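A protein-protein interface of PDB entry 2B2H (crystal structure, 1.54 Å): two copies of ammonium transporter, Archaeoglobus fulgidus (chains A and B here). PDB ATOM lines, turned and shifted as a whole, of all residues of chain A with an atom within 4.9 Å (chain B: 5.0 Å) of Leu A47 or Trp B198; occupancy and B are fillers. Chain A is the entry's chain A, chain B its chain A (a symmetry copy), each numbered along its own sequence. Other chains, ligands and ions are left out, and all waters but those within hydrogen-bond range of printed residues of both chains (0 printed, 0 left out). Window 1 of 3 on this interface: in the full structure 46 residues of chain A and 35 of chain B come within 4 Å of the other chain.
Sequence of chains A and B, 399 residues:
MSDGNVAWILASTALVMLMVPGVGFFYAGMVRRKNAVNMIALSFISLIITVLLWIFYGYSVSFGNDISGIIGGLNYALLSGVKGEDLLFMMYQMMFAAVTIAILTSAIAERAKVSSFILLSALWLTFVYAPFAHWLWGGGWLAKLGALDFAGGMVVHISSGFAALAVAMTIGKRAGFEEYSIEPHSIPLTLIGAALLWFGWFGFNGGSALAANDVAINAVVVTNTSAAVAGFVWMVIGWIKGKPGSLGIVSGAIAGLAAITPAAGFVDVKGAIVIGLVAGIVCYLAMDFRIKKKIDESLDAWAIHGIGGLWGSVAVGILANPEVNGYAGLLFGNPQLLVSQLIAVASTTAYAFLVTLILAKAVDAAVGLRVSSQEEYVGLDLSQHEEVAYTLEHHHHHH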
ATOM      1  N   MET A  17       6.916   5.311  23.736  1.00  0.00           N
ATOM      2  CA  MET A  17       7.069   6.711  24.136  1.00  0.00           C
ATOM      3  C   MET A  17       5.819   7.493  23.741  1.00  0.00           C
ATOM      4  O   MET A  17       5.357   8.354  24.488  1.00  0.00           O
ATOM      5  CB  MET A  17       8.303   7.334  23.468  1.00  0.00           C
ATOM      6  CG  MET A  17       8.405   8.854  23.591  1.00  0.00           C
ATOM      7  SD  MET A  17       7.454   9.735  22.335  1.00  0.00           S
ATOM      8  CE  MET A  17       6.843  11.123  23.296  1.00  0.00           C
ATOM      9  N   VAL A  20       2.809   7.675  26.126  1.00  0.00           N
ATOM     10  CA  VAL A  20       2.793   8.577  27.287  1.00  0.00           C
ATOM     11  C   VAL A  20       1.872   9.769  26.987  1.00  0.00           C
ATOM     12  O   VAL A  20       0.893   9.982  27.713  1.00  0.00           O
ATOM     13  CB  VAL A  20       4.216   9.057  27.671  1.00  0.00           C
ATOM     14  CG1 VAL A  20       4.147   9.973  28.884  1.00  0.00           C
ATOM     15  CG2 VAL A  20       5.094   7.857  27.990  1.00  0.00           C
ATOM     16  N   SER A  43       1.022  14.209  31.628  1.00  0.00           N
ATOM     17  CA  SER A  43       1.646  13.082  30.938  1.00  0.00           C
ATOM     18  C   SER A  43       3.016  13.466  30.381  1.00  0.00           C
ATOM     19  O   SER A  43       3.930  12.642  30.358  1.00  0.00           O
ATOM     20  CB  SER A  43       0.737  12.542  29.821  1.00  0.00           C
ATOM     21  OG  SER A  43       0.563  13.484  28.770  1.00  0.00           O
ATOM     22  N   PHE A  44       3.168  14.711  29.935  1.00  0.00           N
ATOM     23  CA  PHE A  44       4.463  15.150  29.421  1.00  0.00           C
ATOM     24  C   PHE A  44       5.457  15.262  30.584  1.00  0.00           C
ATOM     25  O   PHE A  44       6.637  14.927  30.441  1.00  0.00           O
ATOM     26  CB  PHE A  44       4.353  16.501  28.706  1.00  0.00           C
ATOM     27  CG  PHE A  44       3.983  16.392  27.256  1.00  0.00           C
ATOM     28  CD1 PHE A  44       2.664  16.540  26.846  1.00  0.00           C
ATOM     29  CD2 PHE A  44       4.956  16.124  26.300  1.00  0.00           C
ATOM     30  CE1 PHE A  44       2.316  16.424  25.494  1.00  0.00           C
ATOM     31  CE2 PHE A  44       4.621  16.006  24.954  1.00  0.00           C
ATOM     32  CZ  PHE A  44       3.295  16.158  24.551  1.00  0.00           C
ATOM     33  N   ILE A  45       4.981  15.750  31.730  1.00  0.00           N
ATOM     34  CA  ILE A  45       5.830  15.877  32.908  1.00  0.00           C
ATOM     35  C   ILE A  45       6.209  14.456  33.346  1.00  0.00           C
ATOM     36  O   ILE A  45       7.350  14.203  33.720  1.00  0.00           O
ATOM     37  CB  ILE A  45       5.094  16.635  34.046  1.00  0.00           C
ATOM     38  CG1 ILE A  45       4.851  18.085  33.613  1.00  0.00           C
ATOM     39  CG2 ILE A  45       5.916  16.617  35.319  1.00  0.00           C
ATOM     40  CD1 ILE A  45       3.987  18.892  34.570  1.00  0.00           C
ATOM     41  N   SER A  46       5.258  13.527  33.280  1.00  0.00           N
ATOM     42  CA  SER A  46       5.546  12.143  33.647  1.00  0.00           C
ATOM     43  C   SER A  46       6.710  11.631  32.803  1.00  0.00           C
ATOM     44  O   SER A  46       7.593  10.940  33.302  1.00  0.00           O
ATOM     45  CB  SER A  46       4.323  11.253  33.412  1.00  0.00           C
ATOM     46  OG  SER A  46       3.264  11.581  34.295  1.00  0.00           O
ATOM     47  N   LEU A  47       6.710  11.969  31.517  1.00  0.00           N
ATOM     48  CA  LEU A  47       7.783  11.529  30.633  1.00  0.00           C
ATOM     49  C   LEU A  47       9.120  12.173  31.028  1.00  0.00           C
ATOM     50  O   LEU A  47      10.111  11.468  31.240  1.00  0.00           O
ATOM     51  CB  LEU A  47       7.456  11.867  29.168  1.00  0.00           C
ATOM     52  CG  LEU A  47       8.459  11.384  28.109  1.00  0.00           C
ATOM     53  CD1 LEU A  47       8.593   9.880  28.186  1.00  0.00           C
ATOM     54  CD2 LEU A  47       7.995  11.792  26.715  1.00  0.00           C
ATOM     55  N   ILE A  48       9.139  13.502  31.142  1.00  0.00           N
ATOM     56  CA  ILE A  48      10.356  14.234  31.493  1.00  0.00           C
ATOM     57  C   ILE A  48      10.960  13.782  32.816  1.00  0.00           C
ATOM     58  O   ILE A  48      12.165  13.540  32.902  1.00  0.00           O
ATOM     59  CB  ILE A  48      10.094  15.748  31.558  1.00  0.00           C
ATOM     60  CG1 ILE A  48       9.651  16.245  30.178  1.00  0.00           C
ATOM     61  CG2 ILE A  48      11.357  16.479  32.028  1.00  0.00           C
ATOM     62  CD1 ILE A  48       9.104  17.652  30.163  1.00  0.00           C
ATOM     63  N   ILE A  49      10.124  13.665  33.841  1.00  0.00           N
ATOM     64  CA  ILE A  49      10.587  13.233  35.156  1.00  0.00           C
ATOM     65  C   ILE A  49      11.123  11.797  35.113  1.00  0.00           C
ATOM     66  O   ILE A  49      12.166  11.503  35.699  1.00  0.00           O
ATOM     67  CB  ILE A  49       9.445  13.329  36.215  1.00  0.00           C
ATOM     68  CG1 ILE A  49       9.015  14.787  36.389  1.00  0.00           C
ATOM     69  CG2 ILE A  49       9.898  12.767  37.543  1.00  0.00           C
ATOM     70  CD1 ILE A  49      10.155  15.750  36.614  1.00  0.00           C
ATOM     71  N   THR A  50      10.427  10.908  34.410  1.00  0.00           N
ATOM     72  CA  THR A  50      10.863   9.517  34.326  1.00  0.00           C
ATOM     73  C   THR A  50      12.210   9.349  33.624  1.00  0.00           C
ATOM     74  O   THR A  50      13.059   8.570  34.068  1.00  0.00           O
ATOM     75  CB  THR A  50       9.810   8.654  33.617  1.00  0.00           C
ATOM     76  OG1 THR A  50       8.589   8.704  34.363  1.00  0.00           O
ATOM     77  CG2 THR A  50      10.268   7.207  33.526  1.00  0.00           C
ATOM     78  N   VAL A  51      12.415  10.076  32.531  1.00  0.00           N
ATOM     79  CA  VAL A  51      13.677   9.986  31.800  1.00  0.00           C
ATOM     80  C   VAL A  51      14.855  10.334  32.707  1.00  0.00           C
ATOM     81  O   VAL A  51      15.854   9.617  32.741  1.00  0.00           O
ATOM     82  CB  VAL A  51      13.701  10.936  30.572  1.00  0.00           C
ATOM     83  CG1 VAL A  51      15.117  11.040  30.019  1.00  0.00           C
ATOM     84  CG2 VAL A  51      12.763  10.418  29.492  1.00  0.00           C
ATOM     85  N   MET A  95      10.581   3.776  28.942  1.00  0.00           N
ATOM     86  CA  MET A  95       9.252   4.169  28.462  1.00  0.00           C
ATOM     87  C   MET A  95       8.104   3.429  29.163  1.00  0.00           C
ATOM     88  O   MET A  95       7.003   3.971  29.273  1.00  0.00           O
ATOM     89  CB  MET A  95       9.161   4.001  26.936  1.00  0.00           C
ATOM     90  CG  MET A  95      10.173   4.846  26.146  1.00  0.00           C
ATOM     91  SD  MET A  95      10.094   6.633  26.516  1.00  0.00           S
ATOM     92  CE  MET A  95      11.697   7.183  25.936  1.00  0.00           C
ATOM     93  N   ALA A  98       7.489   5.394  32.238  1.00  0.00           N
ATOM     94  CA  ALA A  98       6.799   6.639  31.907  1.00  0.00           C
ATOM     95  C   ALA A  98       5.302   6.425  31.683  1.00  0.00           C
ATOM     96  O   ALA A  98       4.481   7.182  32.196  1.00  0.00           O
ATOM     97  CB  ALA A  98       7.431   7.272  30.668  1.00  0.00           C
ATOM     98  N   ALA B 194       3.251  18.490  19.518  1.00  0.00           N
ATOM     99  CA  ALA B 194       4.463  18.262  20.290  1.00  0.00           C
ATOM    100  C   ALA B 194       4.702  16.760  20.483  1.00  0.00           C
ATOM    101  O   ALA B 194       5.838  16.292  20.418  1.00  0.00           O
ATOM    102  CB  ALA B 194       4.347  18.960  21.636  1.00  0.00           C
ATOM    103  N   ALA B 195       3.635  16.004  20.725  1.00  0.00           N
ATOM    104  CA  ALA B 195       3.743  14.558  20.906  1.00  0.00           C
ATOM    105  C   ALA B 195       4.251  13.903  19.628  1.00  0.00           C
ATOM    106  O   ALA B 195       5.098  13.015  19.680  1.00  0.00           O
ATOM    107  CB  ALA B 195       2.397  13.970  21.289  1.00  0.00           C
ATOM    108  N   LEU B 196       3.743  14.341  18.480  1.00  0.00           N
ATOM    109  CA  LEU B 196       4.168  13.771  17.198  1.00  0.00           C
ATOM    110  C   LEU B 196       5.612  14.131  16.849  1.00  0.00           C
ATOM    111  O   LEU B 196       6.300  13.367  16.176  1.00  0.00           O
ATOM    112  CB  LEU B 196       3.251  14.236  16.065  1.00  0.00           C
ATOM    113  CG  LEU B 196       1.773  13.851  16.160  1.00  0.00           C
ATOM    114  CD1 LEU B 196       1.073  14.268  14.876  1.00  0.00           C
ATOM    115  CD2 LEU B 196       1.636  12.350  16.384  1.00  0.00           C
ATOM    116  N   LEU B 197       6.064  15.298  17.301  1.00  0.00           N
ATOM    117  CA  LEU B 197       7.425  15.741  17.031  1.00  0.00           C
ATOM    118  C   LEU B 197       8.425  14.977  17.884  1.00  0.00           C
ATOM    119  O   LEU B 197       9.510  14.635  17.410  1.00  0.00           O
ATOM    120  CB  LEU B 197       7.560  17.241  17.292  1.00  0.00           C
ATOM    121  CG  LEU B 197       6.877  18.142  16.256  1.00  0.00           C
ATOM    122  CD1 LEU B 197       6.912  19.581  16.743  1.00  0.00           C
ATOM    123  CD2 LEU B 197       7.578  18.018  14.905  1.00  0.00           C
ATOM    124  N   TRP B 198       8.077  14.710  19.139  1.00  0.00           N
ATOM    125  CA  TRP B 198       8.976  13.961  20.015  1.00  0.00           C
ATOM    126  C   TRP B 198       9.051  12.525  19.471  1.00  0.00           C
ATOM    127  O   TRP B 198      10.135  11.959  19.323  1.00  0.00           O
ATOM    128  CB  TRP B 198       8.443  13.956  21.452  1.00  0.00           C
ATOM    129  CG  TRP B 198       9.438  13.495  22.497  1.00  0.00           C
ATOM    130  CD1 TRP B 198      10.265  12.408  22.421  1.00  0.00           C
ATOM    131  CD2 TRP B 198       9.662  14.076  23.795  1.00  0.00           C
ATOM    132  NE1 TRP B 198      10.988  12.276  23.588  1.00  0.00           N
ATOM    133  CE2 TRP B 198      10.637  13.285  24.447  1.00  0.00           C
ATOM    134  CE3 TRP B 198       9.134  15.187  24.467  1.00  0.00           C
ATOM    135  CZ2 TRP B 198      11.095  13.569  25.744  1.00  0.00           C
ATOM    136  CZ3 TRP B 198       9.591  15.469  25.760  1.00  0.00           C
ATOM    137  CH2 TRP B 198      10.562  14.658  26.380  1.00  0.00           C
ATOM    138  N   PHE B 199       7.895  11.948  19.154  1.00  0.00           N
ATOM    139  CA  PHE B 199       7.821  10.595  18.614  1.00  0.00           C
ATOM    140  C   PHE B 199       8.631  10.468  17.317  1.00  0.00           C
ATOM    141  O   PHE B 199       9.493   9.607  17.198  1.00  0.00           O
ATOM    142  CB  PHE B 199       6.346  10.241  18.373  1.00  0.00           C
ATOM    143  CG  PHE B 199       6.125   8.956  17.610  1.00  0.00           C
ATOM    144  CD1 PHE B 199       6.550   7.735  18.123  1.00  0.00           C
ATOM    145  CD2 PHE B 199       5.453   8.972  16.387  1.00  0.00           C
ATOM    146  CE1 PHE B 199       6.305   6.554  17.430  1.00  0.00           C
ATOM    147  CE2 PHE B 199       5.207   7.800  15.692  1.00  0.00           C
ATOM    148  CZ  PHE B 199       5.632   6.589  16.216  1.00  0.00           C
ATOM    149  N   GLY B 200       8.362  11.334  16.349  1.00  0.00           N
ATOM    150  CA  GLY B 200       9.080  11.272  15.088  1.00  0.00           C
ATOM    151  C   GLY B 200      10.580  11.508  15.182  1.00  0.00           C
ATOM    152  O   GLY B 200      11.345  11.045  14.335  1.00  0.00           O
ATOM    153  N   TRP B 201      11.009  12.231  16.209  1.00  0.00           N
ATOM    154  CA  TRP B 201      12.424  12.522  16.382  1.00  0.00           C
ATOM    155  C   TRP B 201      13.220  11.237  16.637  1.00  0.00           C
ATOM    156  O   TRP B 201      14.443  11.243  16.549  1.00  0.00           O
ATOM    157  CB  TRP B 201      12.622  13.520  17.525  1.00  0.00           C
ATOM    158  CG  TRP B 201      13.610  14.600  17.197  1.00  0.00           C
ATOM    159  CD1 TRP B 201      14.935  14.440  16.892  1.00  0.00           C
ATOM    160  CD2 TRP B 201      13.351  16.008  17.143  1.00  0.00           C
ATOM    161  NE1 TRP B 201      15.519  15.666  16.652  1.00  0.00           N
ATOM    162  CE2 TRP B 201      14.568  16.643  16.800  1.00  0.00           C
ATOM    163  CE3 TRP B 201      12.210  16.795  17.350  1.00  0.00           C
ATOM    164  CZ2 TRP B 201      14.675  18.032  16.660  1.00  0.00           C
ATOM    165  CZ3 TRP B 201      12.315  18.175  17.209  1.00  0.00           C
ATOM    166  CH2 TRP B 201      13.542  18.779  16.866  1.00  0.00           C
ATOM    167  N   PHE B 202      12.525  10.145  16.961  1.00  0.00           N
ATOM    168  CA  PHE B 202      13.186   8.853  17.164  1.00  0.00           C
ATOM    169  C   PHE B 202      13.754   8.456  15.802  1.00  0.00           C
ATOM    170  O   PHE B 202      14.832   7.875  15.711  1.00  0.00           O
ATOM    171  CB  PHE B 202      12.187   7.787  17.632  1.00  0.00           C
ATOM    172  CG  PHE B 202      11.986   7.747  19.126  1.00  0.00           C
ATOM    173  CD1 PHE B 202      12.619   6.781  19.902  1.00  0.00           C
ATOM    174  CD2 PHE B 202      11.175   8.676  19.758  1.00  0.00           C
ATOM    175  CE1 PHE B 202      12.450   6.740  21.291  1.00  0.00           C
ATOM    176  CE2 PHE B 202      11.000   8.642  21.144  1.00  0.00           C
ATOM    177  CZ  PHE B 202      11.641   7.670  21.913  1.00  0.00           C
ATOM    178  N   ASN B 224      16.520  11.592  23.923  1.00  0.00           N
ATOM    179  CA  ASN B 224      15.500  11.648  24.968  1.00  0.00           C
ATOM    180  C   ASN B 224      16.050  12.344  26.208  1.00  0.00           C
ATOM    181  O   ASN B 224      15.326  13.053  26.909  1.00  0.00           O
ATOM    182  CB  ASN B 224      15.034  10.237  25.328  1.00  0.00           C
ATOM    183  CG  ASN B 224      14.016   9.691  24.342  1.00  0.00           C
ATOM    184  OD1 ASN B 224      12.851  10.087  24.364  1.00  0.00           O
ATOM    185  ND2 ASN B 224      14.452   8.789  23.463  1.00  0.00           N
ATOM    186  N   ALA B 227      16.188  16.181  25.636  1.00  0.00           N
ATOM    187  CA  ALA B 227      14.820  16.688  25.584  1.00  0.00           C
ATOM    188  C   ALA B 227      14.277  16.845  27.001  1.00  0.00           C
ATOM    189  O   ALA B 227      13.708  17.882  27.350  1.00  0.00           O
ATOM    190  CB  ALA B 227      13.926  15.731  24.778  1.00  0.00           C
ATOM    191  N   ALA B 228      14.477  15.811  27.814  1.00  0.00           N
ATOM    192  CA  ALA B 228      14.000  15.793  29.194  1.00  0.00           C
ATOM    193  C   ALA B 228      14.638  16.877  30.050  1.00  0.00           C
ATOM    194  O   ALA B 228      13.961  17.545  30.836  1.00  0.00           O
ATOM    195  CB  ALA B 228      14.256  14.417  29.812  1.00  0.00           C
ATOM    196  N   ALA B 253      11.470  21.163  25.736  1.00  0.00           N
ATOM    197  CA  ALA B 253      11.840  19.834  25.250  1.00  0.00           C
ATOM    198  C   ALA B 253      12.337  19.907  23.805  1.00  0.00           C
ATOM    199  O   ALA B 253      13.316  19.258  23.442  1.00  0.00           O
ATOM    200  CB  ALA B 253      10.644  18.884  25.346  1.00  0.00           C
ATOM    201  N   LEU B 257      15.800  18.878  21.997  1.00  0.00           N
ATOM    202  CA  LEU B 257      15.843  17.980  20.847  1.00  0.00           C
ATOM    203  C   LEU B 257      16.635  18.596  19.689  1.00  0.00           C
ATOM    204  O   LEU B 257      17.389  17.906  19.007  1.00  0.00           O
ATOM    205  CB  LEU B 257      14.417  17.641  20.396  1.00  0.00           C
ATOM    206  CG  LEU B 257      13.592  16.795  21.371  1.00  0.00           C
ATOM    207  CD1 LEU B 257      12.126  16.796  20.960  1.00  0.00           C
ATOM    208  CD2 LEU B 257      14.142  15.373  21.389  1.00  0.00           C
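NE1 of Trp B198 lies within hydrogen-bond range of OD1 of Asn B224 (3.0 Å).
Of the printed residues of chain B, Phe A44 touches Ala B195 (3.8 Å). Leu A47 touches one residue of chain B. Of the printed residues of chain B, Ile A48 touches Ala B228. Of the printed residues of chain B, Met A95 touches Asn B224. Of the printed residues of chain A, Phe B202 touches Met A17 (3.6 Å). The nearest printed residue of chain B that does not touch Leu A47 is Ala B228 (5.3 Å).
Of the 14 printed residues of chain B, 6 touch a printed residue of chain A. Among the printed residues, 9 pairs touch across the chains.
Met A17 touches Trp B198 (CE to CG, 3.6 Å). Met A17 touches Phe B199. CG of Met A17 touches CE2 of Phe B202, 3.6 Å away. Phe A44 touches Ala B195 (CZ to N, 3.8 Å). CD2 of Leu A47 touches CZ2 of Trp B198, at 3.7 Å. Ala B228 touches Ile A48. CG1 of Val A51 touches O of Asn B224, at 3.7 Å. Ala B228 touches Val A51. OD1 of Asn B224 touches CE of Met A95 (3.5 Å).
No position is printed for both chains. Of the 9 pairs that touch across the chains among the printed residues, none has its exchanged pair printed and touching as well.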
